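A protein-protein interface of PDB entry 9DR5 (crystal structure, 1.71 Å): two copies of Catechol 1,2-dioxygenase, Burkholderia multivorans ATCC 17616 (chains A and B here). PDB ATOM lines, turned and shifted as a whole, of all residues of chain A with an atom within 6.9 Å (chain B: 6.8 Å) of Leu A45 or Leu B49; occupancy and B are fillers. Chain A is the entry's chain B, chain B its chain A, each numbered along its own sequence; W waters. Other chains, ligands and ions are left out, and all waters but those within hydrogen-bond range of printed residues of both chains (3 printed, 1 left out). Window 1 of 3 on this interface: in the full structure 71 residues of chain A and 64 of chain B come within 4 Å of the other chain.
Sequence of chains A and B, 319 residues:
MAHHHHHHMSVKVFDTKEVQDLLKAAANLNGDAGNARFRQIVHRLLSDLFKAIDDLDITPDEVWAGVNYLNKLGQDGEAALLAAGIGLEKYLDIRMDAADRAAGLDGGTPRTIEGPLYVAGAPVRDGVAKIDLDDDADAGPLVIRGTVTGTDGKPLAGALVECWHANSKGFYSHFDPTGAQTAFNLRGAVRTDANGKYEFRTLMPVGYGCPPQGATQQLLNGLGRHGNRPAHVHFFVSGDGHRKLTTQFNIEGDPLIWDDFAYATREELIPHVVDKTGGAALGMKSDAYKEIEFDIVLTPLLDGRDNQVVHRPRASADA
The backbone NH (N) of Phe B14 sits at hydrogen-bond distance from the side-chain carboxylate (OD2) of Asp B54, at 3.0 Å.
The side-chain carboxylate of Asp A48 is in salt-bridge range of the guanidinium group of Arg A44 (2.8 Å).
NE of Arg B44 is in salt-bridge range of OD2 of Asp B48 (2.8 Å).
The backbone carbonyl oxygen of Ile B53 is in hydrogen-bond range of the backbone NH of Ile B58, 3.0 Å away.
The backbone carbonyl oxygen (O) of Phe B50 lies within hydrogen-bond range of the side-chain hydroxyl (OH) of Tyr A91, at 2.7 Å.
Water W2 lies within hydrogen-bond range of OD2 of Asp B48 (2.5 Å), O of Asp A48 (2.7 Å) and NH2 of Arg B44 (2.9 Å).
Water W3 bridges OD2 of Asp B48 and O of Asp A48.
Water W1 lies within hydrogen-bond range of O of Asp B48, OD2 of Asp A48 and N of Leu B49.
Printed residues of chain B within 4 Å of Leu A45: Leu B49.
Leu B49 touches just one residue of chain A: Leu A45 (3.9 Å).
Printed residues of chain A within 4 Å of Leu B46: Ile A86.
Printed residues of chain B within 4 Å of Arg A44: Lys B51, Ala B52 and Leu B56.
Phe A50 touches none of the printed residues of chain B.
The nearest residue of chain A that does not touch Leu B49 is Leu A88 (4.5 Å).
The nearest printed residue of chain B that does not touch Arg A44 is Asp B48 (5.0 Å).
Among the printed residues, merely in contact across the chains: Ile A41 with Leu B56 (3.9 Å), Arg A44 with Lys B51 (3.9 Å), Arg A44 with Ala B52 (3.7 Å), Arg A44 with Leu B56 (3.5 Å), Leu A45 with Leu B49 (3.9 Å), Asp A48 with Asp B48 (3.8 Å), Asp A48 with Ala B52 (3.9 Å), Leu A49 with Leu B45 (3.9 Å), Ile A86 with Leu B46 (3.8 Å), Ile A86 with Phe B50 (3.8 Å), Leu A88 with Phe B50 (3.8 Å), Leu A88 with Ile B53 (3.6 Å), Tyr A91 with Ile B53 (3.9 Å) and Tyr A91 with Asp B54 (3.4 Å).
Hydrophobic or aromatic side chains of chain B that line the printed part of chain A: Leu B45, Leu B46, Leu B49, Phe B50, Ala B52, Ile B53 and Leu B56.
Printed residues of chain A that touch a printed residue of chain B: Ile A41, Arg A44, Leu A45, Asp A48, Leu A49, Ile A86, Leu A88 and Tyr A91.
Hydrophobic or aromatic side chains of chain A within 4 Å of the printed part of chain B: Leu A45, Leu A49, Ile A86, Leu A88 and Tyr A91.
Along chain A the printed residues that touch a printed residue of chain B span positions 41 to 91.
Among the printed residues, 15 pairs touch across the chains.
Among the printed residues, no Asp or Glu carboxylate lies within 4 Å of a Lys or Arg side-chain nitrogen of the other chain.
Leu A45 touches Leu B49, and with the chains exchanged Leu A49 touches Leu B45.
Asp B48 touches its own counterpart, Asp A48.
Positions printed for both chains: 44, 45, 46, 47, 48, 49 and 50.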
ATOM      1  N   LEU A  23      -3.796  -9.818   4.812  1.00  0.00           N
ATOM      2  CA  LEU A  23      -4.618 -10.336   3.726  1.00  0.00           C
ATOM      3  C   LEU A  23      -5.915  -9.541   3.588  1.00  0.00           C
ATOM      4  O   LEU A  23      -6.365  -9.261   2.467  1.00  0.00           O
ATOM      5  CB  LEU A  23      -4.924 -11.815   3.952  1.00  0.00           C
ATOM      6  CG  LEU A  23      -3.769 -12.771   3.639  1.00  0.00           C
ATOM      7  CD1 LEU A  23      -4.002 -14.118   4.307  1.00  0.00           C
ATOM      8  CD2 LEU A  23      -3.600 -12.925   2.137  1.00  0.00           C
ATOM      9  N   GLN A  40     -13.460 -10.826  -3.199  1.00  0.00           N
ATOM     10  CA  GLN A  40     -13.604 -12.166  -2.635  1.00  0.00           C
ATOM     11  C   GLN A  40     -12.644 -13.147  -3.296  1.00  0.00           C
ATOM     12  O   GLN A  40     -11.998 -13.959  -2.620  1.00  0.00           O
ATOM     13  CB  GLN A  40     -15.061 -12.623  -2.811  1.00  0.00           C
ATOM     14  CG  GLN A  40     -15.349 -14.063  -2.436  1.00  0.00           C
ATOM     15  CD  GLN A  40     -16.715 -14.563  -2.946  1.00  0.00           C
ATOM     16  OE1 GLN A  40     -17.182 -14.177  -4.022  1.00  0.00           O
ATOM     17  NE2 GLN A  40     -17.344 -15.437  -2.173  1.00  0.00           N
ATOM     18  N   ILE A  41     -12.560 -13.105  -4.625  1.00  0.00           N
ATOM     19  CA  ILE A  41     -11.684 -14.013  -5.360  1.00  0.00           C
ATOM     20  C   ILE A  41     -10.224 -13.735  -5.033  1.00  0.00           C
ATOM     21  O   ILE A  41      -9.442 -14.652  -4.755  1.00  0.00           O
ATOM     22  CB  ILE A  41     -11.954 -13.892  -6.868  1.00  0.00           C
ATOM     23  CG1 ILE A  41     -13.328 -14.487  -7.188  1.00  0.00           C
ATOM     24  CG2 ILE A  41     -10.856 -14.576  -7.648  1.00  0.00           C
ATOM     25  CD1 ILE A  41     -13.772 -14.271  -8.629  1.00  0.00           C
ATOM     26  N   VAL A  42      -9.837 -12.457  -5.039  1.00  0.00           N
ATOM     27  CA  VAL A  42      -8.446 -12.102  -4.761  1.00  0.00           C
ATOM     28  C   VAL A  42      -8.054 -12.514  -3.345  1.00  0.00           C
ATOM     29  O   VAL A  42      -6.957 -13.044  -3.121  1.00  0.00           O
ATOM     30  CB  VAL A  42      -8.227 -10.595  -5.018  1.00  0.00           C
ATOM     31  CG1 VAL A  42      -6.925 -10.145  -4.451  1.00  0.00           C
ATOM     32  CG2 VAL A  42      -8.288 -10.321  -6.517  1.00  0.00           C
ATOM     33  N   HIS A  43      -8.940 -12.295  -2.364  1.00  0.00           N
ATOM     34  CA  HIS A  43      -8.624 -12.701  -0.996  1.00  0.00           C
ATOM     35  C   HIS A  43      -8.416 -14.206  -0.899  1.00  0.00           C
ATOM     36  O   HIS A  43      -7.488 -14.673  -0.225  1.00  0.00           O
ATOM     37  CB  HIS A  43      -9.720 -12.269  -0.030  1.00  0.00           C
ATOM     38  CG  HIS A  43      -9.426 -12.618   1.393  1.00  0.00           C
ATOM     39  ND1 HIS A  43      -9.846 -13.792   1.975  1.00  0.00           N
ATOM     40  CD2 HIS A  43      -8.692 -11.974   2.329  1.00  0.00           C
ATOM     41  CE1 HIS A  43      -9.426 -13.830   3.227  1.00  0.00           C
ATOM     42  NE2 HIS A  43      -8.715 -12.743   3.464  1.00  0.00           N
ATOM     43  N   ARG A  44      -9.248 -14.979  -1.588  1.00  0.00           N
ATOM     44  CA  ARG A  44      -9.090 -16.430  -1.561  1.00  0.00           C
ATOM     45  C   ARG A  44      -7.768 -16.858  -2.192  1.00  0.00           C
ATOM     46  O   ARG A  44      -7.019 -17.653  -1.611  1.00  0.00           O
ATOM     47  CB  ARG A  44     -10.285 -17.087  -2.255  1.00  0.00           C
ATOM     48  CG  ARG A  44     -10.153 -18.588  -2.420  1.00  0.00           C
ATOM     49  CD  ARG A  44      -9.923 -19.342  -1.097  1.00  0.00           C
ATOM     50  NE  ARG A  44      -9.842 -20.785  -1.344  1.00  0.00           N
ATOM     51  CZ  ARG A  44     -10.875 -21.615  -1.283  1.00  0.00           C
ATOM     52  NH1 ARG A  44     -12.083 -21.192  -0.954  1.00  0.00           N
ATOM     53  NH2 ARG A  44     -10.689 -22.909  -1.555  1.00  0.00           N
ATOM     54  N   LEU A  45      -7.448 -16.327  -3.378  1.00  0.00           N
ATOM     55  CA  LEU A  45      -6.215 -16.726  -4.053  1.00  0.00           C
ATOM     56  C   LEU A  45      -4.992 -16.302  -3.262  1.00  0.00           C
ATOM     57  O   LEU A  45      -4.021 -17.052  -3.152  1.00  0.00           O
ATOM     58  CB  LEU A  45      -6.175 -16.117  -5.453  1.00  0.00           C
ATOM     59  CG  LEU A  45      -7.292 -16.573  -6.402  1.00  0.00           C
ATOM     60  CD1 LEU A  45      -7.153 -15.893  -7.759  1.00  0.00           C
ATOM     61  CD2 LEU A  45      -7.276 -18.079  -6.565  1.00  0.00           C
ATOM     62  N   LEU A  46      -5.026 -15.095  -2.706  1.00  0.00           N
ATOM     63  CA  LEU A  46      -3.903 -14.594  -1.924  1.00  0.00           C
ATOM     64  C   LEU A  46      -3.737 -15.393  -0.635  1.00  0.00           C
ATOM     65  O   LEU A  46      -2.621 -15.807  -0.289  1.00  0.00           O
ATOM     66  CB  LEU A  46      -4.144 -13.112  -1.641  1.00  0.00           C
ATOM     67  CG  LEU A  46      -2.998 -12.134  -1.527  1.00  0.00           C
ATOM     68  CD1 LEU A  46      -2.033 -12.228  -2.716  1.00  0.00           C
ATOM     69  CD2 LEU A  46      -3.627 -10.754  -1.460  1.00  0.00           C
ATOM     70  N   SER A  47      -4.851 -15.664   0.059  1.00  0.00           N
ATOM     71  CA  SER A  47      -4.800 -16.454   1.285  1.00  0.00           C
ATOM     72  C   SER A  47      -4.224 -17.838   1.014  1.00  0.00           C
ATOM     73  O   SER A  47      -3.357 -18.318   1.754  1.00  0.00           O
ATOM     74  CB  SER A  47      -6.199 -16.558   1.888  1.00  0.00           C
ATOM     75  OG  SER A  47      -6.219 -17.294   3.100  1.00  0.00           O
ATOM     76  N   ASP A  48      -4.693 -18.494  -0.061  1.00  0.00           N
ATOM     77  CA  ASP A  48      -4.188 -19.816  -0.400  1.00  0.00           C
ATOM     78  C   ASP A  48      -2.697 -19.773  -0.732  1.00  0.00           C
ATOM     79  O   ASP A  48      -1.939 -20.657  -0.323  1.00  0.00           O
ATOM     80  CB  ASP A  48      -4.982 -20.390  -1.578  1.00  0.00           C
ATOM     81  CG  ASP A  48      -6.395 -20.822  -1.191  1.00  0.00           C
ATOM     82  OD1 ASP A  48      -6.748 -20.807   0.020  1.00  0.00           O
ATOM     83  OD2 ASP A  48      -7.153 -21.199  -2.118  1.00  0.00           O
ATOM     84  N   LEU A  49      -2.265 -18.767  -1.495  1.00  0.00           N
ATOM     85  CA  LEU A  49      -0.844 -18.615  -1.805  1.00  0.00           C
ATOM     86  C   LEU A  49      -0.008 -18.437  -0.537  1.00  0.00           C
ATOM     87  O   LEU A  49       1.027 -19.100  -0.369  1.00  0.00           O
ATOM     88  CB  LEU A  49      -0.636 -17.428  -2.741  1.00  0.00           C
ATOM     89  CG  LEU A  49       0.830 -17.089  -3.061  1.00  0.00           C
ATOM     90  CD1 LEU A  49       1.519 -18.232  -3.808  1.00  0.00           C
ATOM     91  CD2 LEU A  49       0.930 -15.789  -3.845  1.00  0.00           C
ATOM     92  N   PHE A  50      -0.444 -17.550   0.367  1.00  0.00           N
ATOM     93  CA  PHE A  50       0.305 -17.338   1.606  1.00  0.00           C
ATOM     94  C   PHE A  50       0.370 -18.629   2.427  1.00  0.00           C
ATOM     95  O   PHE A  50       1.415 -18.962   3.002  1.00  0.00           O
ATOM     96  CB  PHE A  50      -0.309 -16.217   2.447  1.00  0.00           C
ATOM     97  CG  PHE A  50      -0.041 -14.797   1.946  1.00  0.00           C
ATOM     98  CD1 PHE A  50       0.326 -14.529   0.641  1.00  0.00           C
ATOM     99  CD2 PHE A  50      -0.219 -13.723   2.806  1.00  0.00           C
ATOM    100  CE1 PHE A  50       0.521 -13.201   0.207  1.00  0.00           C
ATOM    101  CE2 PHE A  50      -0.010 -12.400   2.374  1.00  0.00           C
ATOM    102  CZ  PHE A  50       0.356 -12.158   1.072  1.00  0.00           C
ATOM    103  N   ILE A  86      -1.294 -26.857 -18.069  1.00  0.00           N
ATOM    104  CA  ILE A  86      -1.387 -27.386 -16.709  1.00  0.00           C
ATOM    105  C   ILE A  86      -2.814 -27.820 -16.361  1.00  0.00           C
ATOM    106  O   ILE A  86      -3.140 -28.004 -15.185  1.00  0.00           O
ATOM    107  CB  ILE A  86      -0.809 -26.431 -15.649  1.00  0.00           C
ATOM    108  CG1 ILE A  86      -1.138 -24.976 -15.896  1.00  0.00           C
ATOM    109  CG2 ILE A  86       0.706 -26.642 -15.595  1.00  0.00           C
ATOM    110  CD1 ILE A  86      -2.598 -24.632 -15.752  1.00  0.00           C
ATOM    111  N   LEU A  88      -5.805 -26.530 -16.538  1.00  0.00           N
ATOM    112  CA  LEU A  88      -6.861 -25.610 -16.127  1.00  0.00           C
ATOM    113  C   LEU A  88      -7.980 -25.570 -17.162  1.00  0.00           C
ATOM    114  O   LEU A  88      -9.166 -25.547 -16.816  1.00  0.00           O
ATOM    115  CB  LEU A  88      -6.266 -24.224 -15.908  1.00  0.00           C
ATOM    116  CG  LEU A  88      -7.248 -23.101 -15.612  1.00  0.00           C
ATOM    117  CD1 LEU A  88      -8.027 -23.424 -14.345  1.00  0.00           C
ATOM    118  CD2 LEU A  88      -6.496 -21.773 -15.462  1.00  0.00           C
ATOM    119  N   TYR A  91      -9.964 -28.594 -16.808  1.00  0.00           N
ATOM    120  CA  TYR A  91     -10.719 -28.510 -15.574  1.00  0.00           C
ATOM    121  C   TYR A  91     -12.014 -27.733 -15.769  1.00  0.00           C
ATOM    122  O   TYR A  91     -13.054 -28.104 -15.209  1.00  0.00           O
ATOM    123  CB  TYR A  91      -9.832 -27.877 -14.498  1.00  0.00           C
ATOM    124  CG  TYR A  91     -10.448 -27.783 -13.144  1.00  0.00           C
ATOM    125  CD1 TYR A  91     -10.809 -28.938 -12.445  1.00  0.00           C
ATOM    126  CD2 TYR A  91     -10.649 -26.557 -12.532  1.00  0.00           C
ATOM    127  CE1 TYR A  91     -11.358 -28.864 -11.198  1.00  0.00           C
ATOM    128  CE2 TYR A  91     -11.200 -26.476 -11.267  1.00  0.00           C
ATOM    129  CZ  TYR A  91     -11.561 -27.632 -10.603  1.00  0.00           C
ATOM    130  OH  TYR A  91     -12.100 -27.556  -9.326  1.00  0.00           O
ATOM    131  N   PHE B  14     -13.984 -30.860  -7.084  1.00  0.00           N
ATOM    132  CA  PHE B  14     -12.566 -30.908  -6.747  1.00  0.00           C
ATOM    133  C   PHE B  14     -12.159 -32.253  -6.143  1.00  0.00           C
ATOM    134  O   PHE B  14     -11.116 -32.802  -6.511  1.00  0.00           O
ATOM    135  CB  PHE B  14     -12.191 -29.775  -5.800  1.00  0.00           C
ATOM    136  CG  PHE B  14     -10.747 -29.803  -5.411  1.00  0.00           C
ATOM    137  CD1 PHE B  14      -9.781 -29.380  -6.305  1.00  0.00           C
ATOM    138  CD2 PHE B  14     -10.344 -30.294  -4.169  1.00  0.00           C
ATOM    139  CE1 PHE B  14      -8.448 -29.418  -5.965  1.00  0.00           C
ATOM    140  CE2 PHE B  14      -9.002 -30.316  -3.828  1.00  0.00           C
ATOM    141  CZ  PHE B  14      -8.060 -29.882  -4.735  1.00  0.00           C
ATOM    142  N   ARG B  44       0.841 -28.196  -5.538  1.00  0.00           N
ATOM    143  CA  ARG B  44       0.131 -27.480  -4.485  1.00  0.00           C
ATOM    144  C   ARG B  44      -0.560 -26.238  -5.030  1.00  0.00           C
ATOM    145  O   ARG B  44      -1.721 -25.978  -4.707  1.00  0.00           O
ATOM    146  CB  ARG B  44       1.098 -27.106  -3.357  1.00  0.00           C
ATOM    147  CG  ARG B  44       0.486 -26.208  -2.297  1.00  0.00           C
ATOM    148  CD  ARG B  44      -0.755 -26.829  -1.627  1.00  0.00           C
ATOM    149  NE  ARG B  44      -1.246 -25.985  -0.535  1.00  0.00           N
ATOM    150  CZ  ARG B  44      -0.841 -26.062   0.726  1.00  0.00           C
ATOM    151  NH1 ARG B  44       0.032 -26.980   1.125  1.00  0.00           N
ATOM    152  NH2 ARG B  44      -1.328 -25.200   1.615  1.00  0.00           N
ATOM    153  N   LEU B  45       0.149 -25.435  -5.829  1.00  0.00           N
ATOM    154  CA  LEU B  45      -0.457 -24.223  -6.369  1.00  0.00           C
ATOM    155  C   LEU B  45      -1.621 -24.553  -7.290  1.00  0.00           C
ATOM    156  O   LEU B  45      -2.682 -23.921  -7.218  1.00  0.00           O
ATOM    157  CB  LEU B  45       0.585 -23.394  -7.117  1.00  0.00           C
ATOM    158  CG  LEU B  45       1.701 -22.826  -6.233  1.00  0.00           C
ATOM    159  CD1 LEU B  45       2.710 -22.109  -7.103  1.00  0.00           C
ATOM    160  CD2 LEU B  45       1.158 -21.900  -5.154  1.00  0.00           C
ATOM    161  N   LEU B  46      -1.455 -25.560  -8.148  1.00  0.00           N
ATOM    162  CA  LEU B  46      -2.556 -25.928  -9.032  1.00  0.00           C
ATOM    163  C   LEU B  46      -3.739 -26.473  -8.244  1.00  0.00           C
ATOM    164  O   LEU B  46      -4.889 -26.147  -8.562  1.00  0.00           O
ATOM    165  CB  LEU B  46      -2.112 -26.956 -10.076  1.00  0.00           C
ATOM    166  CG  LEU B  46      -1.220 -26.505 -11.229  1.00  0.00           C
ATOM    167  CD1 LEU B  46      -0.871 -27.715 -12.090  1.00  0.00           C
ATOM    168  CD2 LEU B  46      -1.917 -25.443 -12.071  1.00  0.00           C
ATOM    169  N   SER B  47      -3.486 -27.343  -7.250  1.00  0.00           N
ATOM    170  CA  SER B  47      -4.575 -27.890  -6.442  1.00  0.00           C
ATOM    171  C   SER B  47      -5.345 -26.777  -5.748  1.00  0.00           C
ATOM    172  O   SER B  47      -6.582 -26.752  -5.775  1.00  0.00           O
ATOM    173  CB  SER B  47      -4.043 -28.882  -5.395  1.00  0.00           C
ATOM    174  OG  SER B  47      -3.393 -29.978  -6.001  1.00  0.00           O
ATOM    175  N   ASP B  48      -4.625 -25.821  -5.147  1.00  0.00           N
ATOM    176  CA  ASP B  48      -5.290 -24.717  -4.464  1.00  0.00           C
ATOM    177  C   ASP B  48      -6.115 -23.883  -5.438  1.00  0.00           C
ATOM    178  O   ASP B  48      -7.237 -23.481  -5.121  1.00  0.00           O
ATOM    179  CB  ASP B  48      -4.269 -23.835  -3.741  1.00  0.00           C
ATOM    180  CG  ASP B  48      -3.661 -24.521  -2.507  1.00  0.00           C
ATOM    181  OD1 ASP B  48      -4.182 -25.571  -2.054  1.00  0.00           O
ATOM    182  OD2 ASP B  48      -2.647 -24.003  -1.992  1.00  0.00           O
ATOM    183  N   LEU B  49      -5.573 -23.610  -6.623  1.00  0.00           N
ATOM    184  CA  LEU B  49      -6.321 -22.854  -7.624  1.00  0.00           C
ATOM    185  C   LEU B  49      -7.583 -23.601  -8.035  1.00  0.00           C
ATOM    186  O   LEU B  49      -8.675 -23.023  -8.105  1.00  0.00           O
ATOM    187  CB  LEU B  49      -5.427 -22.609  -8.834  1.00  0.00           C
ATOM    188  CG  LEU B  49      -6.100 -21.896  -9.997  1.00  0.00           C
ATOM    189  CD1 LEU B  49      -6.558 -20.474  -9.607  1.00  0.00           C
ATOM    190  CD2 LEU B  49      -5.156 -21.863 -11.187  1.00  0.00           C
ATOM    191  N   PHE B  50      -7.446 -24.888  -8.361  1.00  0.00           N
ATOM    192  CA  PHE B  50      -8.618 -25.657  -8.775  1.00  0.00           C
ATOM    193  C   PHE B  50      -9.671 -25.667  -7.670  1.00  0.00           C
ATOM    194  O   PHE B  50     -10.871 -25.548  -7.937  1.00  0.00           O
ATOM    195  CB  PHE B  50      -8.236 -27.096  -9.130  1.00  0.00           C
ATOM    196  CG  PHE B  50      -7.524 -27.261 -10.461  1.00  0.00           C
ATOM    197  CD1 PHE B  50      -6.901 -26.204 -11.091  1.00  0.00           C
ATOM    198  CD2 PHE B  50      -7.483 -28.497 -11.064  1.00  0.00           C
ATOM    199  CE1 PHE B  50      -6.247 -26.388 -12.330  1.00  0.00           C
ATOM    200  CE2 PHE B  50      -6.838 -28.688 -12.266  1.00  0.00           C
ATOM    201  CZ  PHE B  50      -6.213 -27.642 -12.900  1.00  0.00           C
ATOM    202  N   LYS B  51      -9.243 -25.822  -6.418  1.00  0.00           N
ATOM    203  CA  LYS B  51     -10.205 -25.861  -5.330  1.00  0.00           C
ATOM    204  C   LYS B  51     -10.873 -24.505  -5.145  1.00  0.00           C
ATOM    205  O   LYS B  51     -12.069 -24.427  -4.852  1.00  0.00           O
ATOM    206  CB  LYS B  51      -9.519 -26.323  -4.046  1.00  0.00           C
ATOM    207  CG  LYS B  51     -10.474 -26.526  -2.884  1.00  0.00           C
ATOM    208  CD  LYS B  51      -9.746 -26.998  -1.625  1.00  0.00           C
ATOM    209  CE  LYS B  51     -10.710 -27.498  -0.546  1.00  0.00           C
ATOM    210  NZ  LYS B  51     -11.750 -26.502  -0.140  1.00  0.00           N
ATOM    211  N   ALA B  52     -10.113 -23.418  -5.298  1.00  0.00           N
ATOM    212  CA  ALA B  52     -10.714 -22.093  -5.182  1.00  0.00           C
ATOM    213  C   ALA B  52     -11.736 -21.849  -6.284  1.00  0.00           C
ATOM    214  O   ALA B  52     -12.788 -21.246  -6.046  1.00  0.00           O
ATOM    215  CB  ALA B  52      -9.622 -21.026  -5.193  1.00  0.00           C
ATOM    216  N   ILE B  53     -11.451 -22.315  -7.505  1.00  0.00           N
ATOM    217  CA  ILE B  53     -12.413 -22.190  -8.593  1.00  0.00           C
ATOM    218  C   ILE B  53     -13.682 -22.956  -8.262  1.00  0.00           C
ATOM    219  O   ILE B  53     -14.799 -22.490  -8.504  1.00  0.00           O
ATOM    220  CB  ILE B  53     -11.783 -22.693  -9.908  1.00  0.00           C
ATOM    221  CG1 ILE B  53     -10.779 -21.665 -10.444  1.00  0.00           C
ATOM    222  CG2 ILE B  53     -12.841 -22.988 -10.946  1.00  0.00           C
ATOM    223  CD1 ILE B  53      -9.895 -22.210 -11.537  1.00  0.00           C
ATOM    224  N   ASP B  54     -13.520 -24.163  -7.736  1.00  0.00           N
ATOM    225  CA  ASP B  54     -14.659 -24.991  -7.350  1.00  0.00           C
ATOM    226  C   ASP B  54     -15.472 -24.335  -6.233  1.00  0.00           C
ATOM    227  O   ASP B  54     -16.706 -24.236  -6.312  1.00  0.00           O
ATOM    228  CB  ASP B  54     -14.120 -26.364  -6.927  1.00  0.00           C
ATOM    229  CG  ASP B  54     -15.148 -27.472  -7.029  1.00  0.00           C
ATOM    230  OD1 ASP B  54     -15.852 -27.551  -8.060  1.00  0.00           O
ATOM    231  OD2 ASP B  54     -15.207 -28.292  -6.096  1.00  0.00           O
ATOM    232  N   LEU B  56     -15.645 -21.186  -5.061  1.00  0.00           N
ATOM    233  CA  LEU B  56     -16.248 -19.898  -5.374  1.00  0.00           C
ATOM    234  C   LEU B  56     -17.046 -19.925  -6.675  1.00  0.00           C
ATOM    235  O   LEU B  56     -17.574 -18.884  -7.079  1.00  0.00           O
ATOM    236  CB  LEU B  56     -15.156 -18.810  -5.440  1.00  0.00           C
ATOM    237  CG  LEU B  56     -14.603 -18.348  -4.095  1.00  0.00           C
ATOM    238  CD1 LEU B  56     -14.051 -19.513  -3.315  1.00  0.00           C
ATOM    239  CD2 LEU B  56     -13.516 -17.307  -4.277  1.00  0.00           C
ATOM    240  N   ILE B  58     -16.049 -20.085  -9.755  1.00  0.00           N
ATOM    241  CA  ILE B  58     -15.482 -19.127 -10.688  1.00  0.00           C
ATOM    242  C   ILE B  58     -15.801 -19.601 -12.100  1.00  0.00           C
ATOM    243  O   ILE B  58     -15.538 -20.760 -12.460  1.00  0.00           O
ATOM    244  CB  ILE B  58     -13.976 -18.964 -10.438  1.00  0.00           C
ATOM    245  CG1 ILE B  58     -13.734 -18.579  -8.970  1.00  0.00           C
ATOM    246  CG2 ILE B  58     -13.405 -17.914 -11.338  1.00  0.00           C
ATOM    247  CD1 ILE B  58     -12.294 -18.303  -8.615  1.00  0.00           C
HETATM  248  O   HOH W   1      -5.915 -20.643  -5.005  1.00  0.00           O
HETATM  249  O   HOH W   2      -2.890 -23.123   0.355  1.00  0.00           O
HETATM  250  O   HOH W   3      -1.614 -21.659  -3.397  1.00  0.00           O
